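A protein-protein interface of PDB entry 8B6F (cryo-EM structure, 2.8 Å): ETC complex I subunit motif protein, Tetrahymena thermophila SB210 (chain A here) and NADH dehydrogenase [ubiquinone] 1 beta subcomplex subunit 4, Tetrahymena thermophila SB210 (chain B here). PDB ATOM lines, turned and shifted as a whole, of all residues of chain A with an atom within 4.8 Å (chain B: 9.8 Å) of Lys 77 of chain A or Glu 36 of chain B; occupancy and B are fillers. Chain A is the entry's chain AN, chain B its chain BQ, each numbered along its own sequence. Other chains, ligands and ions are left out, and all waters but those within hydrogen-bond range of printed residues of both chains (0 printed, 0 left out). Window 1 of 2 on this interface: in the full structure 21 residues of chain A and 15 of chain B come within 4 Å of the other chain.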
ATOM      1  N   GLU A  71     -24.105 -29.703  22.622  1.00  0.00           N
ATOM      2  CA  GLU A  71     -23.975 -28.932  23.852  1.00  0.00           C
ATOM      3  C   GLU A  71     -22.764 -28.007  23.750  1.00  0.00           C
ATOM      4  O   GLU A  71     -21.688 -28.455  23.345  1.00  0.00           O
ATOM      5  CB  GLU A  71     -23.825 -29.867  25.050  1.00  0.00           C
ATOM      6  CG  GLU A  71     -23.675 -29.155  26.383  1.00  0.00           C
ATOM      7  CD  GLU A  71     -24.865 -28.280  26.714  1.00  0.00           C
ATOM      8  OE1 GLU A  71     -25.946 -28.496  26.127  1.00  0.00           O
ATOM      9  OE2 GLU A  71     -24.720 -27.370  27.557  1.00  0.00           O
ATOM     10  N   MET A  73     -21.417 -26.269  26.390  1.00  0.00           N
ATOM     11  CA  MET A  73     -20.703 -26.325  27.666  1.00  0.00           C
ATOM     12  C   MET A  73     -20.950 -27.677  28.320  1.00  0.00           C
ATOM     13  O   MET A  73     -21.625 -27.772  29.352  1.00  0.00           O
ATOM     14  CB  MET A  73     -21.133 -25.178  28.583  1.00  0.00           C
ATOM     15  CG  MET A  73     -20.869 -23.804  27.987  1.00  0.00           C
ATOM     16  SD  MET A  73     -21.429 -22.448  29.029  1.00  0.00           S
ATOM     17  CE  MET A  73     -20.920 -21.046  28.039  1.00  0.00           C
ATOM     18  N   PRO A  74     -20.417 -28.754  27.738  1.00  0.00           N
ATOM     19  CA  PRO A  74     -20.604 -30.074  28.361  1.00  0.00           C
ATOM     20  C   PRO A  74     -20.065 -30.148  29.777  1.00  0.00           C
ATOM     21  O   PRO A  74     -20.692 -30.769  30.641  1.00  0.00           O
ATOM     22  CB  PRO A  74     -19.846 -31.018  27.415  1.00  0.00           C
ATOM     23  CG  PRO A  74     -19.723 -30.275  26.135  1.00  0.00           C
ATOM     24  CD  PRO A  74     -19.621 -28.835  26.503  1.00  0.00           C
ATOM     25  N   ARG A  75     -18.921 -29.516  30.043  1.00  0.00           N
ATOM     26  CA  ARG A  75     -18.361 -29.538  31.390  1.00  0.00           C
ATOM     27  C   ARG A  75     -19.291 -28.852  32.380  1.00  0.00           C
ATOM     28  O   ARG A  75     -19.519 -29.360  33.484  1.00  0.00           O
ATOM     29  CB  ARG A  75     -16.984 -28.879  31.398  1.00  0.00           C
ATOM     30  CG  ARG A  75     -15.908 -29.705  30.714  1.00  0.00           C
ATOM     31  CD  ARG A  75     -14.653 -28.889  30.465  1.00  0.00           C
ATOM     32  NE  ARG A  75     -14.173 -28.225  31.670  1.00  0.00           N
ATOM     33  CZ  ARG A  75     -13.409 -28.796  32.592  1.00  0.00           C
ATOM     34  NH1 ARG A  75     -13.036 -30.060  32.494  1.00  0.00           N
ATOM     35  NH2 ARG A  75     -13.005 -28.078  33.635  1.00  0.00           N
ATOM     36  N   ALA A  76     -19.838 -27.697  32.006  1.00  0.00           N
ATOM     37  CA  ALA A  76     -20.767 -27.007  32.893  1.00  0.00           C
ATOM     38  C   ALA A  76     -22.010 -27.848  33.151  1.00  0.00           C
ATOM     39  O   ALA A  76     -22.484 -27.931  34.290  1.00  0.00           O
ATOM     40  CB  ALA A  76     -21.152 -25.653  32.297  1.00  0.00           C
ATOM     41  N   LYS A  77     -22.554 -28.483  32.111  1.00  0.00           N
ATOM     42  CA  LYS A  77     -23.734 -29.319  32.303  1.00  0.00           C
ATOM     43  C   LYS A  77     -23.439 -30.488  33.233  1.00  0.00           C
ATOM     44  O   LYS A  77     -24.238 -30.795  34.126  1.00  0.00           O
ATOM     45  CB  LYS A  77     -24.254 -29.825  30.957  1.00  0.00           C
ATOM     46  CG  LYS A  77     -25.381 -28.982  30.378  1.00  0.00           C
ATOM     47  CD  LYS A  77     -26.206 -29.770  29.374  1.00  0.00           C
ATOM     48  CE  LYS A  77     -27.378 -28.951  28.856  1.00  0.00           C
ATOM     49  NZ  LYS A  77     -28.178 -29.696  27.845  1.00  0.00           N
ATOM     50  N   ILE A  78     -22.298 -31.154  33.048  1.00  0.00           N
ATOM     51  CA  ILE A  78     -21.958 -32.278  33.916  1.00  0.00           C
ATOM     52  C   ILE A  78     -21.829 -31.806  35.356  1.00  0.00           C
ATOM     53  O   ILE A  78     -22.307 -32.466  36.286  1.00  0.00           O
ATOM     54  CB  ILE A  78     -20.669 -32.969  33.434  1.00  0.00           C
ATOM     55  CG1 ILE A  78     -20.886 -33.589  32.055  1.00  0.00           C
ATOM     56  CG2 ILE A  78     -20.239 -34.041  34.430  1.00  0.00           C
ATOM     57  CD1 ILE A  78     -19.636 -34.158  31.418  1.00  0.00           C
ATOM     58  N   MET A  79     -21.174 -30.665  35.568  1.00  0.00           N
ATOM     59  CA  MET A  79     -21.000 -30.157  36.923  1.00  0.00           C
ATOM     60  C   MET A  79     -22.345 -29.836  37.563  1.00  0.00           C
ATOM     61  O   MET A  79     -22.596 -30.198  38.717  1.00  0.00           O
ATOM     62  CB  MET A  79     -20.107 -28.917  36.901  1.00  0.00           C
ATOM     63  CG  MET A  79     -18.657 -29.209  36.574  1.00  0.00           C
ATOM     64  SD  MET A  79     -17.840 -30.192  37.841  1.00  0.00           S
ATOM     65  CE  MET A  79     -17.442 -31.656  36.900  1.00  0.00           C
ATOM     66  N   LYS A  80     -23.231 -29.166  36.825  1.00  0.00           N
ATOM     67  CA  LYS A  80     -24.539 -28.833  37.380  1.00  0.00           C
ATOM     68  C   LYS A  80     -25.311 -30.095  37.737  1.00  0.00           C
ATOM     69  O   LYS A  80     -25.905 -30.191  38.816  1.00  0.00           O
ATOM     70  CB  LYS A  80     -25.333 -27.984  36.388  1.00  0.00           C
ATOM     71  CG  LYS A  80     -24.772 -26.593  36.168  1.00  0.00           C
ATOM     72  CD  LYS A  80     -25.603 -25.835  35.148  1.00  0.00           C
ATOM     73  CE  LYS A  80     -24.999 -24.479  34.841  1.00  0.00           C
ATOM     74  NZ  LYS A  80     -25.799 -23.736  33.829  1.00  0.00           N
ATOM     75  N   ILE A  81     -25.310 -31.079  36.838  1.00  0.00           N
ATOM     76  CA  ILE A  81     -26.037 -32.318  37.094  1.00  0.00           C
ATOM     77  C   ILE A  81     -25.458 -33.025  38.311  1.00  0.00           C
ATOM     78  O   ILE A  81     -26.196 -33.523  39.168  1.00  0.00           O
ATOM     79  CB  ILE A  81     -26.013 -33.221  35.848  1.00  0.00           C
ATOM     80  CG1 ILE A  81     -26.754 -32.547  34.692  1.00  0.00           C
ATOM     81  CG2 ILE A  81     -26.645 -34.571  36.153  1.00  0.00           C
ATOM     82  CD1 ILE A  81     -26.576 -33.242  33.358  1.00  0.00           C
ATOM     83  N   ILE A 135     -24.569 -36.785  28.398  1.00  0.00           N
ATOM     84  CA  ILE A 135     -25.246 -35.770  29.202  1.00  0.00           C
ATOM     85  C   ILE A 135     -26.711 -36.139  29.388  1.00  0.00           C
ATOM     86  O   ILE A 135     -27.256 -36.062  30.495  1.00  0.00           O
ATOM     87  CB  ILE A 135     -25.100 -34.384  28.548  1.00  0.00           C
ATOM     88  CG1 ILE A 135     -23.626 -33.979  28.435  1.00  0.00           C
ATOM     89  CG2 ILE A 135     -25.910 -33.339  29.317  1.00  0.00           C
ATOM     90  CD1 ILE A 135     -23.035 -33.381  29.673  1.00  0.00           C
ATOM     91  N   PRO B  30     -26.530 -25.199  41.669  1.00  0.00           N
ATOM     92  CA  PRO B  30     -27.049 -24.253  40.676  1.00  0.00           C
ATOM     93  C   PRO B  30     -28.381 -24.726  40.114  1.00  0.00           C
ATOM     94  O   PRO B  30     -28.599 -25.920  39.900  1.00  0.00           O
ATOM     95  CB  PRO B  30     -25.956 -24.230  39.603  1.00  0.00           C
ATOM     96  CG  PRO B  30     -25.276 -25.542  39.734  1.00  0.00           C
ATOM     97  CD  PRO B  30     -25.313 -25.880  41.195  1.00  0.00           C
ATOM     98  N   THR B  31     -29.273 -23.771  39.867  1.00  0.00           N
ATOM     99  CA  THR B  31     -30.590 -24.102  39.343  1.00  0.00           C
ATOM    100  C   THR B  31     -30.463 -24.772  37.982  1.00  0.00           C
ATOM    101  O   THR B  31     -29.718 -24.308  37.115  1.00  0.00           O
ATOM    102  CB  THR B  31     -31.451 -22.843  39.230  1.00  0.00           C
ATOM    103  OG1 THR B  31     -30.843 -21.921  38.317  1.00  0.00           O
ATOM    104  CG2 THR B  31     -31.613 -22.180  40.591  1.00  0.00           C
ATOM    105  N   ILE B  32     -31.190 -25.870  37.798  1.00  0.00           N
ATOM    106  CA  ILE B  32     -31.225 -26.593  36.534  1.00  0.00           C
ATOM    107  C   ILE B  32     -32.687 -26.791  36.155  1.00  0.00           C
ATOM    108  O   ILE B  32     -33.461 -27.363  36.929  1.00  0.00           O
ATOM    109  CB  ILE B  32     -30.478 -27.937  36.618  1.00  0.00           C
ATOM    110  CG1 ILE B  32     -30.447 -28.608  35.244  1.00  0.00           C
ATOM    111  CG2 ILE B  32     -31.115 -28.857  37.661  1.00  0.00           C
ATOM    112  CD1 ILE B  32     -29.609 -29.865  35.194  1.00  0.00           C
ATOM    113  N   GLY B  33     -33.070 -26.288  34.980  1.00  0.00           N
ATOM    114  CA  GLY B  33     -34.441 -26.390  34.535  1.00  0.00           C
ATOM    115  C   GLY B  33     -34.698 -27.615  33.676  1.00  0.00           C
ATOM    116  O   GLY B  33     -33.780 -28.242  33.154  1.00  0.00           O
ATOM    117  N   GLN B  34     -35.983 -27.949  33.535  1.00  0.00           N
ATOM    118  CA  GLN B  34     -36.360 -29.084  32.700  1.00  0.00           C
ATOM    119  C   GLN B  34     -35.938 -28.875  31.254  1.00  0.00           C
ATOM    120  O   GLN B  34     -35.657 -29.847  30.543  1.00  0.00           O
ATOM    121  CB  GLN B  34     -37.870 -29.317  32.780  1.00  0.00           C
ATOM    122  CG  GLN B  34     -38.375 -29.691  34.170  1.00  0.00           C
ATOM    123  CD  GLN B  34     -37.760 -30.978  34.698  1.00  0.00           C
ATOM    124  OE1 GLN B  34     -37.430 -31.078  35.879  1.00  0.00           O
ATOM    125  NE2 GLN B  34     -37.612 -31.971  33.827  1.00  0.00           N
ATOM    126  N   VAL B  35     -35.891 -27.622  30.800  1.00  0.00           N
ATOM    127  CA  VAL B  35     -35.506 -27.345  29.419  1.00  0.00           C
ATOM    128  C   VAL B  35     -34.072 -27.789  29.165  1.00  0.00           C
ATOM    129  O   VAL B  35     -33.759 -28.353  28.109  1.00  0.00           O
ATOM    130  CB  VAL B  35     -35.706 -25.851  29.098  1.00  0.00           C
ATOM    131  CG1 VAL B  35     -34.823 -24.974  29.983  1.00  0.00           C
ATOM    132  CG2 VAL B  35     -35.423 -25.583  27.627  1.00  0.00           C
ATOM    133  N   GLU B  36     -33.177 -27.546  30.125  1.00  0.00           N
ATOM    134  CA  GLU B  36     -31.768 -27.860  29.917  1.00  0.00           C
ATOM    135  C   GLU B  36     -31.565 -29.348  29.665  1.00  0.00           C
ATOM    136  O   GLU B  36     -30.765 -29.737  28.806  1.00  0.00           O
ATOM    137  CB  GLU B  36     -30.948 -27.404  31.122  1.00  0.00           C
ATOM    138  CG  GLU B  36     -31.075 -25.918  31.419  1.00  0.00           C
ATOM    139  CD  GLU B  36     -30.162 -25.467  32.542  1.00  0.00           C
ATOM    140  OE1 GLU B  36     -29.243 -26.231  32.906  1.00  0.00           O
ATOM    141  OE2 GLU B  36     -30.364 -24.351  33.065  1.00  0.00           O
ATOM    142  N   LEU B  37     -32.282 -30.197  30.400  1.00  0.00           N
ATOM    143  CA  LEU B  37     -32.139 -31.638  30.246  1.00  0.00           C
ATOM    144  C   LEU B  37     -32.666 -32.149  28.912  1.00  0.00           C
ATOM    145  O   LEU B  37     -32.417 -33.311  28.576  1.00  0.00           O
ATOM    146  CB  LEU B  37     -32.862 -32.355  31.388  1.00  0.00           C
ATOM    147  CG  LEU B  37     -32.416 -31.977  32.801  1.00  0.00           C
ATOM    148  CD1 LEU B  37     -33.252 -32.701  33.843  1.00  0.00           C
ATOM    149  CD2 LEU B  37     -30.942 -32.286  32.999  1.00  0.00           C
ATOM    150  N   GLU B  38     -33.383 -31.324  28.153  1.00  0.00           N
ATOM    151  CA  GLU B  38     -33.943 -31.779  26.894  1.00  0.00           C
ATOM    152  C   GLU B  38     -32.834 -32.025  25.870  1.00  0.00           C
ATOM    153  O   GLU B  38     -31.766 -31.412  25.940  1.00  0.00           O
ATOM    154  CB  GLU B  38     -34.929 -30.750  26.348  1.00  0.00           C
ATOM    155  CG  GLU B  38     -36.056 -30.408  27.306  1.00  0.00           C
ATOM    156  CD  GLU B  38     -36.903 -31.612  27.672  1.00  0.00           C
ATOM    157  OE1 GLU B  38     -36.846 -32.626  26.947  1.00  0.00           O
ATOM    158  OE2 GLU B  38     -37.625 -31.544  28.689  1.00  0.00           O
ATOM    159  N   PRO B  39     -33.063 -32.924  24.908  1.00  0.00           N
ATOM    160  CA  PRO B  39     -31.997 -33.220  23.936  1.00  0.00           C
ATOM    161  C   PRO B  39     -31.750 -32.098  22.943  1.00  0.00           C
ATOM    162  O   PRO B  39     -30.590 -31.815  22.621  1.00  0.00           O
ATOM    163  CB  PRO B  39     -32.503 -34.496  23.247  1.00  0.00           C
ATOM    164  CG  PRO B  39     -33.980 -34.430  23.375  1.00  0.00           C
ATOM    165  CD  PRO B  39     -34.262 -33.751  24.686  1.00  0.00           C
ATOM    166  N   PHE B  40     -32.800 -31.454  22.440  1.00  0.00           N
ATOM    167  CA  PHE B  40     -32.664 -30.380  21.467  1.00  0.00           C
ATOM    168  C   PHE B  40     -33.366 -29.128  21.977  1.00  0.00           C
ATOM    169  O   PHE B  40     -34.303 -29.203  22.776  1.00  0.00           O
ATOM    170  CB  PHE B  40     -33.233 -30.790  20.099  1.00  0.00           C
ATOM    171  CG  PHE B  40     -34.715 -31.016  20.098  1.00  0.00           C
ATOM    172  CD1 PHE B  40     -35.242 -32.227  20.510  1.00  0.00           C
ATOM    173  CD2 PHE B  40     -35.580 -30.025  19.666  1.00  0.00           C
ATOM    174  CE1 PHE B  40     -36.606 -32.443  20.505  1.00  0.00           C
ATOM    175  CE2 PHE B  40     -36.944 -30.233  19.658  1.00  0.00           C
ATOM    176  CZ  PHE B  40     -37.458 -31.445  20.077  1.00  0.00           C
ATOM    177  N   LYS B  41     -32.896 -27.974  21.508  1.00  0.00           N
ATOM    178  CA  LYS B  41     -33.356 -26.679  21.984  1.00  0.00           C
ATOM    179  C   LYS B  41     -34.007 -25.892  20.856  1.00  0.00           C
ATOM    180  O   LYS B  41     -33.617 -26.005  19.691  1.00  0.00           O
ATOM    181  CB  LYS B  41     -32.195 -25.857  22.558  1.00  0.00           C
ATOM    182  CG  LYS B  41     -31.416 -26.547  23.664  1.00  0.00           C
ATOM    183  CD  LYS B  41     -32.244 -26.680  24.926  1.00  0.00           C
ATOM    184  CE  LYS B  41     -31.426 -27.269  26.060  1.00  0.00           C
ATOM    185  NZ  LYS B  41     -30.955 -28.648  25.755  1.00  0.00           N
ATOM    186  N   PHE B  42     -35.006 -25.089  21.216  1.00  0.00           N
ATOM    187  CA  PHE B  42     -35.615 -24.141  20.299  1.00  0.00           C
ATOM    188  C   PHE B  42     -34.919 -22.784  20.422  1.00  0.00           C
ATOM    189  O   PHE B  42     -33.940 -22.626  21.152  1.00  0.00           O
ATOM    190  CB  PHE B  42     -37.115 -24.024  20.575  1.00  0.00           C
ATOM    191  CG  PHE B  42     -37.917 -25.221  20.137  1.00  0.00           C
ATOM    192  CD1 PHE B  42     -37.630 -25.880  18.951  1.00  0.00           C
ATOM    193  CD2 PHE B  42     -38.968 -25.680  20.911  1.00  0.00           C
ATOM    194  CE1 PHE B  42     -38.372 -26.974  18.551  1.00  0.00           C
ATOM    195  CE2 PHE B  42     -39.715 -26.772  20.516  1.00  0.00           C
ATOM    196  CZ  PHE B  42     -39.416 -27.421  19.336  1.00  0.00           C
ATOM    197  N   GLU B  45     -35.324 -21.228  23.974  1.00  0.00           N
ATOM    198  CA  GLU B  45     -34.538 -22.027  24.907  1.00  0.00           C
ATOM    199  C   GLU B  45     -33.046 -21.787  24.713  1.00  0.00           C
ATOM    200  O   GLU B  45     -32.294 -21.695  25.688  1.00  0.00           O
ATOM    201  CB  GLU B  45     -34.882 -23.506  24.736  1.00  0.00           C
ATOM    202  CG  GLU B  45     -36.371 -23.800  24.871  1.00  0.00           C
ATOM    203  CD  GLU B  45     -36.713 -25.247  24.588  1.00  0.00           C
ATOM    204  OE1 GLU B  45     -35.930 -25.918  23.886  1.00  0.00           O
ATOM    205  OE2 GLU B  45     -37.766 -25.717  25.067  1.00  0.00           O
ATOM    206  N   ARG B  46     -32.602 -21.682  23.459  1.00  0.00           N
ATOM    207  CA  ARG B  46     -31.192 -21.415  23.190  1.00  0.00           C
ATOM    208  C   ARG B  46     -30.781 -20.038  23.691  1.00  0.00           C
ATOM    209  O   ARG B  46     -29.667 -19.862  24.193  1.00  0.00           O
ATOM    210  CB  ARG B  46     -30.910 -21.524  21.693  1.00  0.00           C
ATOM    211  CG  ARG B  46     -30.812 -22.939  21.172  1.00  0.00           C
ATOM    212  CD  ARG B  46     -30.562 -22.936  19.674  1.00  0.00           C
ATOM    213  NE  ARG B  46     -30.346 -24.278  19.151  1.00  0.00           N
ATOM    214  CZ  ARG B  46     -30.141 -24.558  17.873  1.00  0.00           C
ATOM    215  NH1 ARG B  46     -30.126 -23.609  16.952  1.00  0.00           N
ATOM    216  NH2 ARG B  46     -29.946 -25.822  17.507  1.00  0.00           N
ATOM    217  N   GLN B  48     -31.693 -18.229  26.286  1.00  0.00           N
ATOM    218  CA  GLN B  48     -31.383 -18.173  27.710  1.00  0.00           C
ATOM    219  C   GLN B  48     -30.016 -18.778  28.001  1.00  0.00           C
ATOM    220  O   GLN B  48     -29.239 -18.226  28.788  1.00  0.00           O
ATOM    221  CB  GLN B  48     -32.469 -18.894  28.507  1.00  0.00           C
ATOM    222  CG  GLN B  48     -33.856 -18.300  28.324  1.00  0.00           C
ATOM    223  CD  GLN B  48     -34.936 -19.132  28.980  1.00  0.00           C
ATOM    224  OE1 GLN B  48     -34.710 -20.284  29.348  1.00  0.00           O
ATOM    225  NE2 GLN B  48     -36.118 -18.548  29.139  1.00  0.00           N
ATOM    226  N   LEU B  49     -29.705 -19.916  27.378  1.00  0.00           N
ATOM    227  CA  LEU B  49     -28.427 -20.576  27.628  1.00  0.00           C
ATOM    228  C   LEU B  49     -27.255 -19.767  27.082  1.00  0.00           C
ATOM    229  O   LEU B  49     -26.212 -19.660  27.738  1.00  0.00           O
ATOM    230  CB  LEU B  49     -28.433 -21.978  27.021  1.00  0.00           C
ATOM    231  CG  LEU B  49     -29.018 -23.087  27.901  1.00  0.00           C
ATOM    232  CD1 LEU B  49     -30.456 -22.787  28.293  1.00  0.00           C
ATOM    233  CD2 LEU B  49     -28.924 -24.431  27.197  1.00  0.00           C
ATOM    234  N   ILE B  50     -27.402 -19.190  25.892  1.00  0.00           N
ATOM    235  CA  ILE B  50     -26.289 -18.514  25.235  1.00  0.00           C
ATOM    236  C   ILE B  50     -26.270 -17.039  25.608  1.00  0.00           C
ATOM    237  O   ILE B  50     -25.514 -16.256  25.024  1.00  0.00           O
ATOM    238  CB  ILE B  50     -26.351 -18.679  23.704  1.00  0.00           C
ATOM    239  CG1 ILE B  50     -27.473 -17.812  23.119  1.00  0.00           C
ATOM    240  CG2 ILE B  50     -26.529 -20.152  23.346  1.00  0.00           C
ATOM    241  CD1 ILE B  50     -27.729 -18.019  21.638  1.00  0.00           C
ATOM    242  N   TYR B  59     -21.245 -22.207  19.288  1.00  0.00           N
ATOM    243  CA  TYR B  59     -21.336 -23.374  18.422  1.00  0.00           C
ATOM    244  C   TYR B  59     -20.378 -23.324  17.241  1.00  0.00           C
ATOM    245  O   TYR B  59     -20.223 -24.336  16.550  1.00  0.00           O
ATOM    246  CB  TYR B  59     -22.766 -23.526  17.898  1.00  0.00           C
ATOM    247  CG  TYR B  59     -23.807 -23.669  18.981  1.00  0.00           C
ATOM    248  CD1 TYR B  59     -24.387 -22.552  19.566  1.00  0.00           C
ATOM    249  CD2 TYR B  59     -24.218 -24.923  19.411  1.00  0.00           C
ATOM    250  CE1 TYR B  59     -25.344 -22.681  20.554  1.00  0.00           C
ATOM    251  CE2 TYR B  59     -25.172 -25.062  20.398  1.00  0.00           C
ATOM    252  CZ  TYR B  59     -25.732 -23.937  20.965  1.00  0.00           C
ATOM    253  OH  TYR B  59     -26.683 -24.073  21.948  1.00  0.00           O
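The backbone carbonyl oxygen (O) of Glu 36 of chain B sits at hydrogen-bond distance from the side-chain amino group (NZ) of Lys 77 of chain A (2.8 Å).
The backbone carbonyl oxygen (O) of Glu 38 of chain B lies within hydrogen-bond range of the side-chain amino group (NZ) of Lys 41 of chain B, 2.9 Å away.
NZ of Lys 41 of chain B is in hydrogen-bond range of O of Glu 36 of chain B, at 3.2 Å.
The side-chain carboxylate (OE1) of Glu 71 of chain A is in salt-bridge range of the side-chain amino group (NZ) of Lys 77 of chain A (3.1 Å).
Among the printed residues, merely in contact across the chains: Lys 77 of chain A with Lys 41 of chain B (3.6 Å), Lys 80 of chain A with Pro 30 of chain B (3.8 Å) and Ile 81 of chain A with Ile 32 of chain B (3.9 Å).
Of the printed residues of chain B, Lys 77 of chain A touches Glu 36 (2.8 Å) and Lys 41 (3.6 Å).
Glu 36 of chain B touches one residue of chain A.
No residue of chain B comes within 4 Å of Ile 78 of chain A.
Lys 80 of chain A touches just one residue of chain B: Pro 30 (3.8 Å).
Of the printed residues of chain A, Ile 32 of chain B touches Ile 81 (3.9 Å).
Of the printed residues of chain A, Pro 30 of chain B touches Lys 80 (3.8 Å).
Printed residues of chain B within 4 Å of Ile 81 of chain A: Ile 32.
Printed residues of chain A within 4 Å of Lys 41 of chain B: Lys 77.
Printed residues of chain B that touch a printed residue of chain A: Pro 30, Ile 32, Glu 36 and Lys 41.
Hydrophobic or aromatic side chains of chain B within 4 Å of the printed part of chain A: Pro 30 and Ile 32.
Of the 11 printed residues of chain A, 3 touch a printed residue of chain B.
Among the printed residues, 4 pairs touch across the chains.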
